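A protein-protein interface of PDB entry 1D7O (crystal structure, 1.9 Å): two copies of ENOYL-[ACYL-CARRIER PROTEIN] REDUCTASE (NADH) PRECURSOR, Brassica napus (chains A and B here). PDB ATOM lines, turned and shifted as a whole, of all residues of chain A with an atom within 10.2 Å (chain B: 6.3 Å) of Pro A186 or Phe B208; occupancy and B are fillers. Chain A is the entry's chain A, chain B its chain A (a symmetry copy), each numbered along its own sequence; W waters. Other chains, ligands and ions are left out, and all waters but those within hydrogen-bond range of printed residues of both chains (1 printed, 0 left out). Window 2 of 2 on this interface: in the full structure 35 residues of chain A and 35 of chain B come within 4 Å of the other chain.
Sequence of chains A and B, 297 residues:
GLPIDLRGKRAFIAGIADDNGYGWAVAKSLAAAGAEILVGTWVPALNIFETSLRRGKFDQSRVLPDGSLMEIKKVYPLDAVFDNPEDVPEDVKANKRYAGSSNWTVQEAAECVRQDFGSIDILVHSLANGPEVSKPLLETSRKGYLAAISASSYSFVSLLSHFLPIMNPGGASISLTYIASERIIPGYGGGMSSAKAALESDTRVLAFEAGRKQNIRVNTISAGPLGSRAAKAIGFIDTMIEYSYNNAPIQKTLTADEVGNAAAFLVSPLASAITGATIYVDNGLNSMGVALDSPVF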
ATOM      1  N   VAL A 133     -21.767  29.387  -7.482  1.00  0.00           N
ATOM      2  CA  VAL A 133     -20.586  28.942  -6.791  1.00  0.00           C
ATOM      3  C   VAL A 133     -20.314  27.446  -6.883  1.00  0.00           C
ATOM      4  O   VAL A 133     -19.181  26.999  -6.827  1.00  0.00           O
ATOM      5  CB  VAL A 133     -20.592  29.443  -5.379  1.00  0.00           C
ATOM      6  CG1 VAL A 133     -21.770  28.860  -4.637  1.00  0.00           C
ATOM      7  CG2 VAL A 133     -19.301  29.049  -4.686  1.00  0.00           C
ATOM      8  N   SER A 134     -21.338  26.631  -7.058  1.00  0.00           N
ATOM      9  CA  SER A 134     -21.057  25.204  -7.154  1.00  0.00           C
ATOM     10  C   SER A 134     -20.692  24.731  -8.549  1.00  0.00           C
ATOM     11  O   SER A 134     -20.497  23.552  -8.771  1.00  0.00           O
ATOM     12  CB  SER A 134     -22.241  24.391  -6.658  1.00  0.00           C
ATOM     13  OG  SER A 134     -23.353  24.554  -7.510  1.00  0.00           O
ATOM     14  N   LYS A 135     -20.644  25.625  -9.514  1.00  0.00           N
ATOM     15  CA  LYS A 135     -20.310  25.227 -10.886  1.00  0.00           C
ATOM     16  C   LYS A 135     -18.837  25.503 -11.228  1.00  0.00           C
ATOM     17  O   LYS A 135     -18.294  26.498 -10.799  1.00  0.00           O
ATOM     18  CB  LYS A 135     -21.103  26.116 -11.881  1.00  0.00           C
ATOM     19  CG  LYS A 135     -22.641  26.052 -11.883  1.00  0.00           C
ATOM     20  CD  LYS A 135     -23.163  24.860 -12.669  1.00  0.00           C
ATOM     21  CE  LYS A 135     -24.689  24.891 -12.780  1.00  0.00           C
ATOM     22  NZ  LYS A 135     -25.217  23.659 -13.434  1.00  0.00           N
ATOM     23  N   PRO A 136     -18.220  24.691 -12.072  1.00  0.00           N
ATOM     24  CA  PRO A 136     -16.847  24.992 -12.460  1.00  0.00           C
ATOM     25  C   PRO A 136     -16.933  26.254 -13.332  1.00  0.00           C
ATOM     26  O   PRO A 136     -17.999  26.595 -13.864  1.00  0.00           O
ATOM     27  CB  PRO A 136     -16.478  23.839 -13.398  1.00  0.00           C
ATOM     28  CG  PRO A 136     -17.613  22.933 -13.399  1.00  0.00           C
ATOM     29  CD  PRO A 136     -18.568  23.300 -12.343  1.00  0.00           C
ATOM     30  N   LEU A 137     -15.813  26.942 -13.508  1.00  0.00           N
ATOM     31  CA  LEU A 137     -15.839  28.115 -14.339  1.00  0.00           C
ATOM     32  C   LEU A 137     -16.277  27.787 -15.754  1.00  0.00           C
ATOM     33  O   LEU A 137     -16.937  28.595 -16.393  1.00  0.00           O
ATOM     34  CB  LEU A 137     -14.460  28.773 -14.433  1.00  0.00           C
ATOM     35  CG  LEU A 137     -14.067  29.863 -13.457  1.00  0.00           C
ATOM     36  CD1 LEU A 137     -12.751  30.435 -14.016  1.00  0.00           C
ATOM     37  CD2 LEU A 137     -15.145  30.937 -13.356  1.00  0.00           C
ATOM     38  N   LEU A 138     -15.871  26.637 -16.274  1.00  0.00           N
ATOM     39  CA  LEU A 138     -16.248  26.313 -17.644  1.00  0.00           C
ATOM     40  C   LEU A 138     -17.763  26.215 -17.762  1.00  0.00           C
ATOM     41  O   LEU A 138     -18.286  26.280 -18.865  1.00  0.00           O
ATOM     42  CB  LEU A 138     -15.614  24.994 -18.086  1.00  0.00           C
ATOM     43  CG  LEU A 138     -14.115  25.011 -18.346  1.00  0.00           C
ATOM     44  CD1 LEU A 138     -13.613  23.589 -18.641  1.00  0.00           C
ATOM     45  CD2 LEU A 138     -13.913  25.933 -19.552  1.00  0.00           C
ATOM     46  N   TYR A 178      -9.973  35.174   0.127  1.00  0.00           N
ATOM     47  CA  TYR A 178      -9.662  33.769   0.286  1.00  0.00           C
ATOM     48  C   TYR A 178      -8.686  33.426  -0.812  1.00  0.00           C
ATOM     49  O   TYR A 178      -8.746  34.018  -1.878  1.00  0.00           O
ATOM     50  CB  TYR A 178     -10.955  32.964   0.186  1.00  0.00           C
ATOM     51  CG  TYR A 178     -10.718  31.484   0.268  1.00  0.00           C
ATOM     52  CD1 TYR A 178     -10.113  30.933   1.398  1.00  0.00           C
ATOM     53  CD2 TYR A 178     -11.086  30.649  -0.773  1.00  0.00           C
ATOM     54  CE1 TYR A 178      -9.879  29.571   1.492  1.00  0.00           C
ATOM     55  CE2 TYR A 178     -10.865  29.289  -0.701  1.00  0.00           C
ATOM     56  CZ  TYR A 178     -10.257  28.762   0.436  1.00  0.00           C
ATOM     57  OH  TYR A 178     -10.011  27.411   0.493  1.00  0.00           O
ATOM     58  N   ILE A 179      -7.780  32.493  -0.528  1.00  0.00           N
ATOM     59  CA  ILE A 179      -6.671  32.074  -1.416  1.00  0.00           C
ATOM     60  C   ILE A 179      -7.023  31.603  -2.820  1.00  0.00           C
ATOM     61  O   ILE A 179      -6.164  31.557  -3.697  1.00  0.00           O
ATOM     62  CB  ILE A 179      -5.767  31.005  -0.698  1.00  0.00           C
ATOM     63  CG1 ILE A 179      -4.412  30.850  -1.376  1.00  0.00           C
ATOM     64  CG2 ILE A 179      -6.427  29.649  -0.723  1.00  0.00           C
ATOM     65  CD1 ILE A 179      -3.398  31.780  -0.891  1.00  0.00           C
ATOM     66  N   ALA A 180      -8.293  31.276  -3.044  1.00  0.00           N
ATOM     67  CA  ALA A 180      -8.714  30.831  -4.372  1.00  0.00           C
ATOM     68  C   ALA A 180      -8.441  31.924  -5.413  1.00  0.00           C
ATOM     69  O   ALA A 180      -8.431  31.686  -6.624  1.00  0.00           O
ATOM     70  CB  ALA A 180     -10.208  30.484  -4.338  1.00  0.00           C
ATOM     71  N   SER A 181      -8.213  33.148  -4.950  1.00  0.00           N
ATOM     72  CA  SER A 181      -7.902  34.192  -5.895  1.00  0.00           C
ATOM     73  C   SER A 181      -6.492  33.957  -6.532  1.00  0.00           C
ATOM     74  O   SER A 181      -6.260  34.249  -7.699  1.00  0.00           O
ATOM     75  CB  SER A 181      -7.816  35.500  -5.127  1.00  0.00           C
ATOM     76  OG  SER A 181      -6.823  35.376  -4.128  1.00  0.00           O
ATOM     77  N   ARG A 183      -4.455  30.850  -6.033  1.00  0.00           N
ATOM     78  CA  ARG A 183      -4.124  29.451  -6.280  1.00  0.00           C
ATOM     79  C   ARG A 183      -5.408  28.726  -6.604  1.00  0.00           C
ATOM     80  O   ARG A 183      -6.490  29.177  -6.248  1.00  0.00           O
ATOM     81  CB  ARG A 183      -3.606  28.848  -4.977  1.00  0.00           C
ATOM     82  CG  ARG A 183      -2.472  29.715  -4.437  1.00  0.00           C
ATOM     83  CD  ARG A 183      -1.102  29.149  -4.669  1.00  0.00           C
ATOM     84  NE  ARG A 183      -0.838  28.325  -3.507  1.00  0.00           N
ATOM     85  CZ  ARG A 183      -0.155  28.761  -2.465  1.00  0.00           C
ATOM     86  NH1 ARG A 183       0.349  29.996  -2.502  1.00  0.00           N
ATOM     87  NH2 ARG A 183       0.019  27.963  -1.418  1.00  0.00           N
ATOM     88  N   ILE A 184      -5.267  27.606  -7.296  1.00  0.00           N
ATOM     89  CA  ILE A 184      -6.402  26.811  -7.714  1.00  0.00           C
ATOM     90  C   ILE A 184      -6.998  26.014  -6.574  1.00  0.00           C
ATOM     91  O   ILE A 184      -6.326  25.132  -5.991  1.00  0.00           O
ATOM     92  CB  ILE A 184      -5.968  25.851  -8.843  1.00  0.00           C
ATOM     93  CG1 ILE A 184      -5.328  26.636  -9.971  1.00  0.00           C
ATOM     94  CG2 ILE A 184      -7.146  24.985  -9.337  1.00  0.00           C
ATOM     95  CD1 ILE A 184      -4.584  25.717 -10.939  1.00  0.00           C
ATOM     96  N   ILE A 185      -8.272  26.289  -6.285  1.00  0.00           N
ATOM     97  CA  ILE A 185      -8.996  25.565  -5.227  1.00  0.00           C
ATOM     98  C   ILE A 185     -10.246  24.998  -5.925  1.00  0.00           C
ATOM     99  O   ILE A 185     -11.254  25.704  -6.142  1.00  0.00           O
ATOM    100  CB  ILE A 185      -9.485  26.483  -4.056  1.00  0.00           C
ATOM    101  CG1 ILE A 185      -8.315  27.179  -3.308  1.00  0.00           C
ATOM    102  CG2 ILE A 185     -10.303  25.660  -3.051  1.00  0.00           C
ATOM    103  CD1 ILE A 185      -7.415  26.207  -2.556  1.00  0.00           C
ATOM    104  N   PRO A 186     -10.202  23.731  -6.298  1.00  0.00           N
ATOM    105  CA  PRO A 186     -11.386  23.151  -6.968  1.00  0.00           C
ATOM    106  C   PRO A 186     -12.558  23.229  -5.981  1.00  0.00           C
ATOM    107  O   PRO A 186     -12.382  23.054  -4.770  1.00  0.00           O
ATOM    108  CB  PRO A 186     -10.976  21.700  -7.247  1.00  0.00           C
ATOM    109  CG  PRO A 186      -9.468  21.741  -7.250  1.00  0.00           C
ATOM    110  CD  PRO A 186      -9.128  22.739  -6.139  1.00  0.00           C
ATOM    111  N   GLY A 187     -13.746  23.517  -6.510  1.00  0.00           N
ATOM    112  CA  GLY A 187     -14.960  23.650  -5.706  1.00  0.00           C
ATOM    113  C   GLY A 187     -15.345  25.113  -5.375  1.00  0.00           C
ATOM    114  O   GLY A 187     -16.470  25.382  -4.976  1.00  0.00           O
ATOM    115  N   TYR A 188     -14.441  26.073  -5.509  1.00  0.00           N
ATOM    116  CA  TYR A 188     -14.818  27.473  -5.201  1.00  0.00           C
ATOM    117  C   TYR A 188     -15.103  28.044  -6.604  1.00  0.00           C
ATOM    118  O   TYR A 188     -14.249  28.707  -7.232  1.00  0.00           O
ATOM    119  CB  TYR A 188     -13.603  28.135  -4.546  1.00  0.00           C
ATOM    120  CG  TYR A 188     -13.873  29.401  -3.794  1.00  0.00           C
ATOM    121  CD1 TYR A 188     -14.410  29.360  -2.516  1.00  0.00           C
ATOM    122  CD2 TYR A 188     -13.571  30.644  -4.356  1.00  0.00           C
ATOM    123  CE1 TYR A 188     -14.614  30.523  -1.820  1.00  0.00           C
ATOM    124  CE2 TYR A 188     -13.791  31.811  -3.675  1.00  0.00           C
ATOM    125  CZ  TYR A 188     -14.303  31.737  -2.412  1.00  0.00           C
ATOM    126  OH  TYR A 188     -14.521  32.883  -1.710  1.00  0.00           O
ATOM    127  N   GLY A 189     -16.299  27.729  -7.111  1.00  0.00           N
ATOM    128  CA  GLY A 189     -16.698  28.083  -8.463  1.00  0.00           C
ATOM    129  C   GLY A 189     -17.535  29.286  -8.672  1.00  0.00           C
ATOM    130  O   GLY A 189     -17.576  30.145  -7.815  1.00  0.00           O
ATOM    131  N   GLY A 190     -18.193  29.332  -9.837  1.00  0.00           N
ATOM    132  CA  GLY A 190     -19.085  30.420 -10.200  1.00  0.00           C
ATOM    133  C   GLY A 190     -18.493  31.824 -10.279  1.00  0.00           C
ATOM    134  O   GLY A 190     -19.229  32.792 -10.225  1.00  0.00           O
ATOM    135  N   SER A 193     -13.802  32.789  -7.351  1.00  0.00           N
ATOM    136  CA  SER A 193     -12.339  32.925  -7.319  1.00  0.00           C
ATOM    137  C   SER A 193     -11.990  34.253  -8.025  1.00  0.00           C
ATOM    138  O   SER A 193     -11.133  35.038  -7.583  1.00  0.00           O
ATOM    139  CB  SER A 193     -11.660  31.768  -8.050  1.00  0.00           C
ATOM    140  OG  SER A 193     -12.150  31.594  -9.369  1.00  0.00           O
ATOM    141  N   GLY A 235     -19.061  18.195   2.120  1.00  0.00           N
ATOM    142  CA  GLY A 235     -19.310  19.576   1.748  1.00  0.00           C
ATOM    143  C   GLY A 235     -17.958  20.259   1.656  1.00  0.00           C
ATOM    144  O   GLY A 235     -16.981  19.830   2.287  1.00  0.00           O
ATOM    145  N   PHE A 236     -17.942  21.296   0.881  1.00  0.00           N
ATOM    146  CA  PHE A 236     -16.725  22.039   0.584  1.00  0.00           C
ATOM    147  C   PHE A 236     -15.987  22.519   1.855  1.00  0.00           C
ATOM    148  O   PHE A 236     -14.788  22.274   2.035  1.00  0.00           O
ATOM    149  CB  PHE A 236     -17.075  23.237  -0.284  1.00  0.00           C
ATOM    150  CG  PHE A 236     -15.889  24.153  -0.527  1.00  0.00           C
ATOM    151  CD1 PHE A 236     -14.889  23.782  -1.433  1.00  0.00           C
ATOM    152  CD2 PHE A 236     -15.810  25.361   0.162  1.00  0.00           C
ATOM    153  CE1 PHE A 236     -13.801  24.633  -1.650  1.00  0.00           C
ATOM    154  CE2 PHE A 236     -14.723  26.214  -0.054  1.00  0.00           C
ATOM    155  CZ  PHE A 236     -13.718  25.850  -0.961  1.00  0.00           C
ATOM    156  N   ILE A 237     -16.695  23.197   2.740  1.00  0.00           N
ATOM    157  CA  ILE A 237     -16.064  23.796   3.939  1.00  0.00           C
ATOM    158  C   ILE A 237     -15.554  22.736   4.940  1.00  0.00           C
ATOM    159  O   ILE A 237     -14.464  22.870   5.516  1.00  0.00           O
ATOM    160  CB  ILE A 237     -17.037  24.747   4.629  1.00  0.00           C
ATOM    161  CG1 ILE A 237     -17.387  25.944   3.740  1.00  0.00           C
ATOM    162  CG2 ILE A 237     -16.475  25.332   5.929  1.00  0.00           C
ATOM    163  CD1 ILE A 237     -18.347  26.931   4.401  1.00  0.00           C
ATOM    164  N   THR A 239     -14.570  19.662   4.389  1.00  0.00           N
ATOM    165  CA  THR A 239     -13.388  19.008   3.907  1.00  0.00           C
ATOM    166  C   THR A 239     -12.164  19.953   4.008  1.00  0.00           C
ATOM    167  O   THR A 239     -11.059  19.499   4.264  1.00  0.00           O
ATOM    168  CB  THR A 239     -13.609  18.429   2.470  1.00  0.00           C
ATOM    169  OG1 THR A 239     -13.673  19.470   1.492  1.00  0.00           O
ATOM    170  CG2 THR A 239     -14.924  17.675   2.427  1.00  0.00           C
ATOM    171  N   MET A 240     -12.383  21.251   3.796  1.00  0.00           N
ATOM    172  CA  MET A 240     -11.299  22.227   3.826  1.00  0.00           C
ATOM    173  C   MET A 240     -10.787  22.460   5.225  1.00  0.00           C
ATOM    174  O   MET A 240      -9.639  22.802   5.437  1.00  0.00           O
ATOM    175  CB  MET A 240     -11.734  23.532   3.161  1.00  0.00           C
ATOM    176  CG  MET A 240     -12.088  23.399   1.703  1.00  0.00           C
ATOM    177  SD  MET A 240     -10.684  22.808   0.685  1.00  0.00           S
ATOM    178  CE  MET A 240      -9.469  23.888   1.445  1.00  0.00           C
ATOM    179  N   TYR A 243      -8.620  19.400   5.802  1.00  0.00           N
ATOM    180  CA  TYR A 243      -7.403  19.512   5.005  1.00  0.00           C
ATOM    181  C   TYR A 243      -6.400  20.505   5.623  1.00  0.00           C
ATOM    182  O   TYR A 243      -5.204  20.221   5.739  1.00  0.00           O
ATOM    183  CB  TYR A 243      -7.768  19.971   3.605  1.00  0.00           C
ATOM    184  CG  TYR A 243      -6.572  20.105   2.726  1.00  0.00           C
ATOM    185  CD1 TYR A 243      -5.770  21.231   2.785  1.00  0.00           C
ATOM    186  CD2 TYR A 243      -6.250  19.115   1.825  1.00  0.00           C
ATOM    187  CE1 TYR A 243      -4.627  21.367   1.946  1.00  0.00           C
ATOM    188  CE2 TYR A 243      -5.148  19.230   0.990  1.00  0.00           C
ATOM    189  CZ  TYR A 243      -4.351  20.358   1.058  1.00  0.00           C
ATOM    190  OH  TYR A 243      -3.286  20.450   0.234  1.00  0.00           O
ATOM    191  N   THR B 203      -7.053  32.295 -15.457  1.00  0.00           N
ATOM    192  CA  THR B 203      -6.078  31.574 -16.254  1.00  0.00           C
ATOM    193  C   THR B 203      -5.625  30.352 -15.480  1.00  0.00           C
ATOM    194  O   THR B 203      -5.489  29.281 -16.021  1.00  0.00           O
ATOM    195  CB  THR B 203      -4.855  32.461 -16.541  1.00  0.00           C
ATOM    196  OG1 THR B 203      -5.281  33.587 -17.321  1.00  0.00           O
ATOM    197  CG2 THR B 203      -3.716  31.659 -17.247  1.00  0.00           C
ATOM    198  N   ARG B 204      -5.388  30.527 -14.192  1.00  0.00           N
ATOM    199  CA  ARG B 204      -4.953  29.431 -13.354  1.00  0.00           C
ATOM    200  C   ARG B 204      -6.057  28.403 -13.217  1.00  0.00           C
ATOM    201  O   ARG B 204      -5.868  27.218 -13.474  1.00  0.00           O
ATOM    202  CB  ARG B 204      -4.594  29.975 -11.973  1.00  0.00           C
ATOM    203  CG  ARG B 204      -3.272  30.770 -12.008  1.00  0.00           C
ATOM    204  CD  ARG B 204      -2.852  31.206 -10.619  1.00  0.00           C
ATOM    205  NE  ARG B 204      -3.662  32.300 -10.090  1.00  0.00           N
ATOM    206  CZ  ARG B 204      -3.425  33.583 -10.346  1.00  0.00           C
ATOM    207  NH1 ARG B 204      -2.393  33.896 -11.122  1.00  0.00           N
ATOM    208  NH2 ARG B 204      -4.210  34.547  -9.838  1.00  0.00           N
ATOM    209  N   VAL B 205      -7.229  28.869 -12.810  1.00  0.00           N
ATOM    210  CA  VAL B 205      -8.348  27.965 -12.642  1.00  0.00           C
ATOM    211  C   VAL B 205      -8.652  27.175 -13.928  1.00  0.00           C
ATOM    212  O   VAL B 205      -8.855  25.966 -13.896  1.00  0.00           O
ATOM    213  CB  VAL B 205      -9.600  28.727 -12.161  1.00  0.00           C
ATOM    214  CG1 VAL B 205     -10.790  27.748 -12.122  1.00  0.00           C
ATOM    215  CG2 VAL B 205      -9.354  29.310 -10.741  1.00  0.00           C
ATOM    216  N   LEU B 206      -8.681  27.856 -15.061  1.00  0.00           N
ATOM    217  CA  LEU B 206      -8.946  27.173 -16.349  1.00  0.00           C
ATOM    218  C   LEU B 206      -7.838  26.231 -16.773  1.00  0.00           C
ATOM    219  O   LEU B 206      -8.116  25.270 -17.477  1.00  0.00           O
ATOM    220  CB  LEU B 206      -9.344  28.140 -17.458  1.00  0.00           C
ATOM    221  CG  LEU B 206     -10.673  28.871 -17.114  1.00  0.00           C
ATOM    222  CD1 LEU B 206     -10.878  30.079 -18.083  1.00  0.00           C
ATOM    223  CD2 LEU B 206     -11.911  27.934 -17.127  1.00  0.00           C
ATOM    224  N   ALA B 207      -6.598  26.483 -16.333  1.00  0.00           N
ATOM    225  CA  ALA B 207      -5.482  25.552 -16.656  1.00  0.00           C
ATOM    226  C   ALA B 207      -5.851  24.170 -15.985  1.00  0.00           C
ATOM    227  O   ALA B 207      -5.680  23.103 -16.555  1.00  0.00           O
ATOM    228  CB  ALA B 207      -4.142  26.084 -16.127  1.00  0.00           C
ATOM    229  N   PHE B 208      -6.382  24.213 -14.775  1.00  0.00           N
ATOM    230  CA  PHE B 208      -6.784  23.002 -14.114  1.00  0.00           C
ATOM    231  C   PHE B 208      -8.028  22.386 -14.821  1.00  0.00           C
ATOM    232  O   PHE B 208      -8.028  21.239 -15.248  1.00  0.00           O
ATOM    233  CB  PHE B 208      -7.116  23.331 -12.655  1.00  0.00           C
ATOM    234  CG  PHE B 208      -7.861  22.230 -11.951  1.00  0.00           C
ATOM    235  CD1 PHE B 208      -7.231  21.012 -11.679  1.00  0.00           C
ATOM    236  CD2 PHE B 208      -9.183  22.407 -11.572  1.00  0.00           C
ATOM    237  CE1 PHE B 208      -7.908  19.980 -11.044  1.00  0.00           C
ATOM    238  CE2 PHE B 208      -9.883  21.399 -10.942  1.00  0.00           C
ATOM    239  CZ  PHE B 208      -9.246  20.171 -10.680  1.00  0.00           C
ATOM    240  N   GLU B 209      -9.093  23.167 -14.979  1.00  0.00           N
ATOM    241  CA  GLU B 209     -10.318  22.657 -15.616  1.00  0.00           C
ATOM    242  C   GLU B 209     -10.108  22.137 -17.048  1.00  0.00           C
ATOM    243  O   GLU B 209     -10.488  21.008 -17.403  1.00  0.00           O
ATOM    244  CB  GLU B 209     -11.481  23.688 -15.574  1.00  0.00           C
ATOM    245  CG  GLU B 209     -11.917  24.115 -14.158  1.00  0.00           C
ATOM    246  CD  GLU B 209     -13.146  24.996 -14.138  1.00  0.00           C
ATOM    247  OE1 GLU B 209     -13.835  25.119 -15.170  1.00  0.00           O
ATOM    248  OE2 GLU B 209     -13.430  25.524 -13.043  1.00  0.00           O
ATOM    249  N   ALA B 210      -9.510  22.960 -17.881  1.00  0.00           N
ATOM    250  CA  ALA B 210      -9.278  22.533 -19.244  1.00  0.00           C
ATOM    251  C   ALA B 210      -8.136  21.550 -19.330  1.00  0.00           C
ATOM    252  O   ALA B 210      -8.106  20.689 -20.202  1.00  0.00           O
ATOM    253  CB  ALA B 210      -9.003  23.707 -20.081  1.00  0.00           C
ATOM    254  N   GLY B 211      -7.190  21.663 -18.416  1.00  0.00           N
ATOM    255  CA  GLY B 211      -6.044  20.745 -18.444  1.00  0.00           C
ATOM    256  C   GLY B 211      -6.497  19.342 -18.160  1.00  0.00           C
ATOM    257  O   GLY B 211      -6.188  18.411 -18.873  1.00  0.00           O
ATOM    258  N   ARG B 212      -7.246  19.186 -17.090  1.00  0.00           N
ATOM    259  CA  ARG B 212      -7.729  17.858 -16.750  1.00  0.00           C
ATOM    260  C   ARG B 212      -8.809  17.410 -17.714  1.00  0.00           C
ATOM    261  O   ARG B 212      -8.987  16.222 -17.938  1.00  0.00           O
ATOM    262  CB  ARG B 212      -8.301  17.809 -15.334  1.00  0.00           C
ATOM    263  CG  ARG B 212      -7.254  17.930 -14.196  1.00  0.00           C
ATOM    264  CD  ARG B 212      -6.196  16.803 -14.290  1.00  0.00           C
ATOM    265  NE  ARG B 212      -5.132  16.874 -13.293  1.00  0.00           N
ATOM    266  CZ  ARG B 212      -4.942  15.981 -12.336  1.00  0.00           C
ATOM    267  NH1 ARG B 212      -5.751  14.943 -12.236  1.00  0.00           N
ATOM    268  NH2 ARG B 212      -3.938  16.117 -11.490  1.00  0.00           N
ATOM    269  N   LYS B 213      -9.557  18.347 -18.269  1.00  0.00           N
ATOM    270  CA  LYS B 213     -10.615  17.936 -19.161  1.00  0.00           C
ATOM    271  C   LYS B 213     -10.207  17.616 -20.538  1.00  0.00           C
ATOM    272  O   LYS B 213     -10.749  16.699 -21.127  1.00  0.00           O
ATOM    273  CB  LYS B 213     -11.809  18.894 -19.186  1.00  0.00           C
ATOM    274  CG  LYS B 213     -12.952  18.418 -20.122  1.00  0.00           C
ATOM    275  CD  LYS B 213     -14.205  19.286 -20.000  1.00  0.00           C
ATOM    276  CE  LYS B 213     -14.932  19.126 -18.641  1.00  0.00           C
ATOM    277  NZ  LYS B 213     -15.723  17.858 -18.429  1.00  0.00           N
ATOM    278  N   VAL B 218      -3.195  26.501 -20.600  1.00  0.00           N
ATOM    279  CA  VAL B 218      -3.750  27.872 -20.543  1.00  0.00           C
ATOM    280  C   VAL B 218      -2.759  28.798 -19.812  1.00  0.00           C
ATOM    281  O   VAL B 218      -2.430  28.554 -18.653  1.00  0.00           O
ATOM    282  CB  VAL B 218      -5.066  27.854 -19.740  1.00  0.00           C
ATOM    283  CG1 VAL B 218      -5.702  29.264 -19.662  1.00  0.00           C
ATOM    284  CG2 VAL B 218      -6.050  26.843 -20.373  1.00  0.00           C
ATOM    285  N   THR B 275       1.836  25.649 -17.989  1.00  0.00           N
ATOM    286  CA  THR B 275       0.401  25.949 -17.990  1.00  0.00           C
ATOM    287  C   THR B 275       0.034  26.657 -16.683  1.00  0.00           C
ATOM    288  O   THR B 275       0.699  26.429 -15.662  1.00  0.00           O
ATOM    289  CB  THR B 275      -0.467  24.645 -18.221  1.00  0.00           C
ATOM    290  OG1 THR B 275      -1.817  25.008 -18.508  1.00  0.00           O
ATOM    291  CG2 THR B 275      -0.485  23.776 -16.980  1.00  0.00           C
HETATM  292  O   HOH W   1      -6.348  31.294  -9.117  1.00  0.00           O
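Glu B209 touches Pro A136.
Leu A137 touches Val B205 (CD1 to CG1, 3.8 Å).
Leu A137 touches Leu B206.
Leu A138 touches Leu B206 (CD2 to CD2, 3.7 Å).
Ile A184 touches Arg B204.
CB of Phe B208 touches CG2 of Ile A184, at 3.7 Å.
Pro A186 touches Phe B208.
Ser A193 touches Val B205.
Printed residues of chain B that touch a printed residue of chain A: Arg B204, Val B205, Leu B206, Phe B208 and Glu B209.
Hydrophobic or aromatic side chains of chain B that line the printed part of chain A: Val B205, Leu B206 and Phe B208.
Printed residues of chain A that touch a printed residue of chain B: Pro A136, Leu A137, Leu A138, Ser A181, Ile A184, Pro A186 and Ser A193.
Hydrophobic or aromatic side chains of chain A that line the printed part of chain B: Pro A136, Leu A137, Leu A138, Ile A184 and Pro A186.
Among the printed residues, 11 pairs touch across the chains.
Among the printed residues, no Asp or Glu carboxylate lies within 4 Å of a Lys or Arg side-chain nitrogen of the other chain.
The backbone NH (N) of Leu A137 sits at hydrogen-bond distance from the side-chain carboxylate (OE2) of Glu B209.
The side-chain carboxylate (OE1) of Glu B209 is in hydrogen-bond range of the backbone NH (N) of Leu A138 (2.8 Å).
The guanidinium group of Arg B204 sits at hydrogen-bond distance from the backbone carbonyl oxygen of Ser A181, at 3.0 Å.
The backbone carbonyl oxygen (O) of Tyr A178 is in hydrogen-bond range of the side-chain hydroxyl (OG) of Ser A181, at 3.3 Å.
No position is printed for both chains.
Of the 11 pairs that touch across the chains among the printed residues, none has its exchanged pair printed and touching as well.
Of the printed residues of chain B, Pro A186 touches Phe B208 (3.7 Å).
Phe B208 touches two residues of chain A.
No residue of chain A comes within 4 Å of Gly B211.
No residue of chain A comes within 4 Å of Arg B212.
Printed residues of chain A within 4 Å of Val B205: Leu A137 and Ser A193.
Printed residues of chain B within 4 Å of Ser A181: Arg B204 (3.0 Å).
The nearest residue of chain A that does not touch Phe B208 is Ile A185 (6.2 Å).
The nearest printed residue of chain A that does not touch Val B205 is Ile A184 (4.1 Å).
Water W1 lies within hydrogen-bond range of NE of Arg B204, O of Ala A180 and O of Ser A181.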
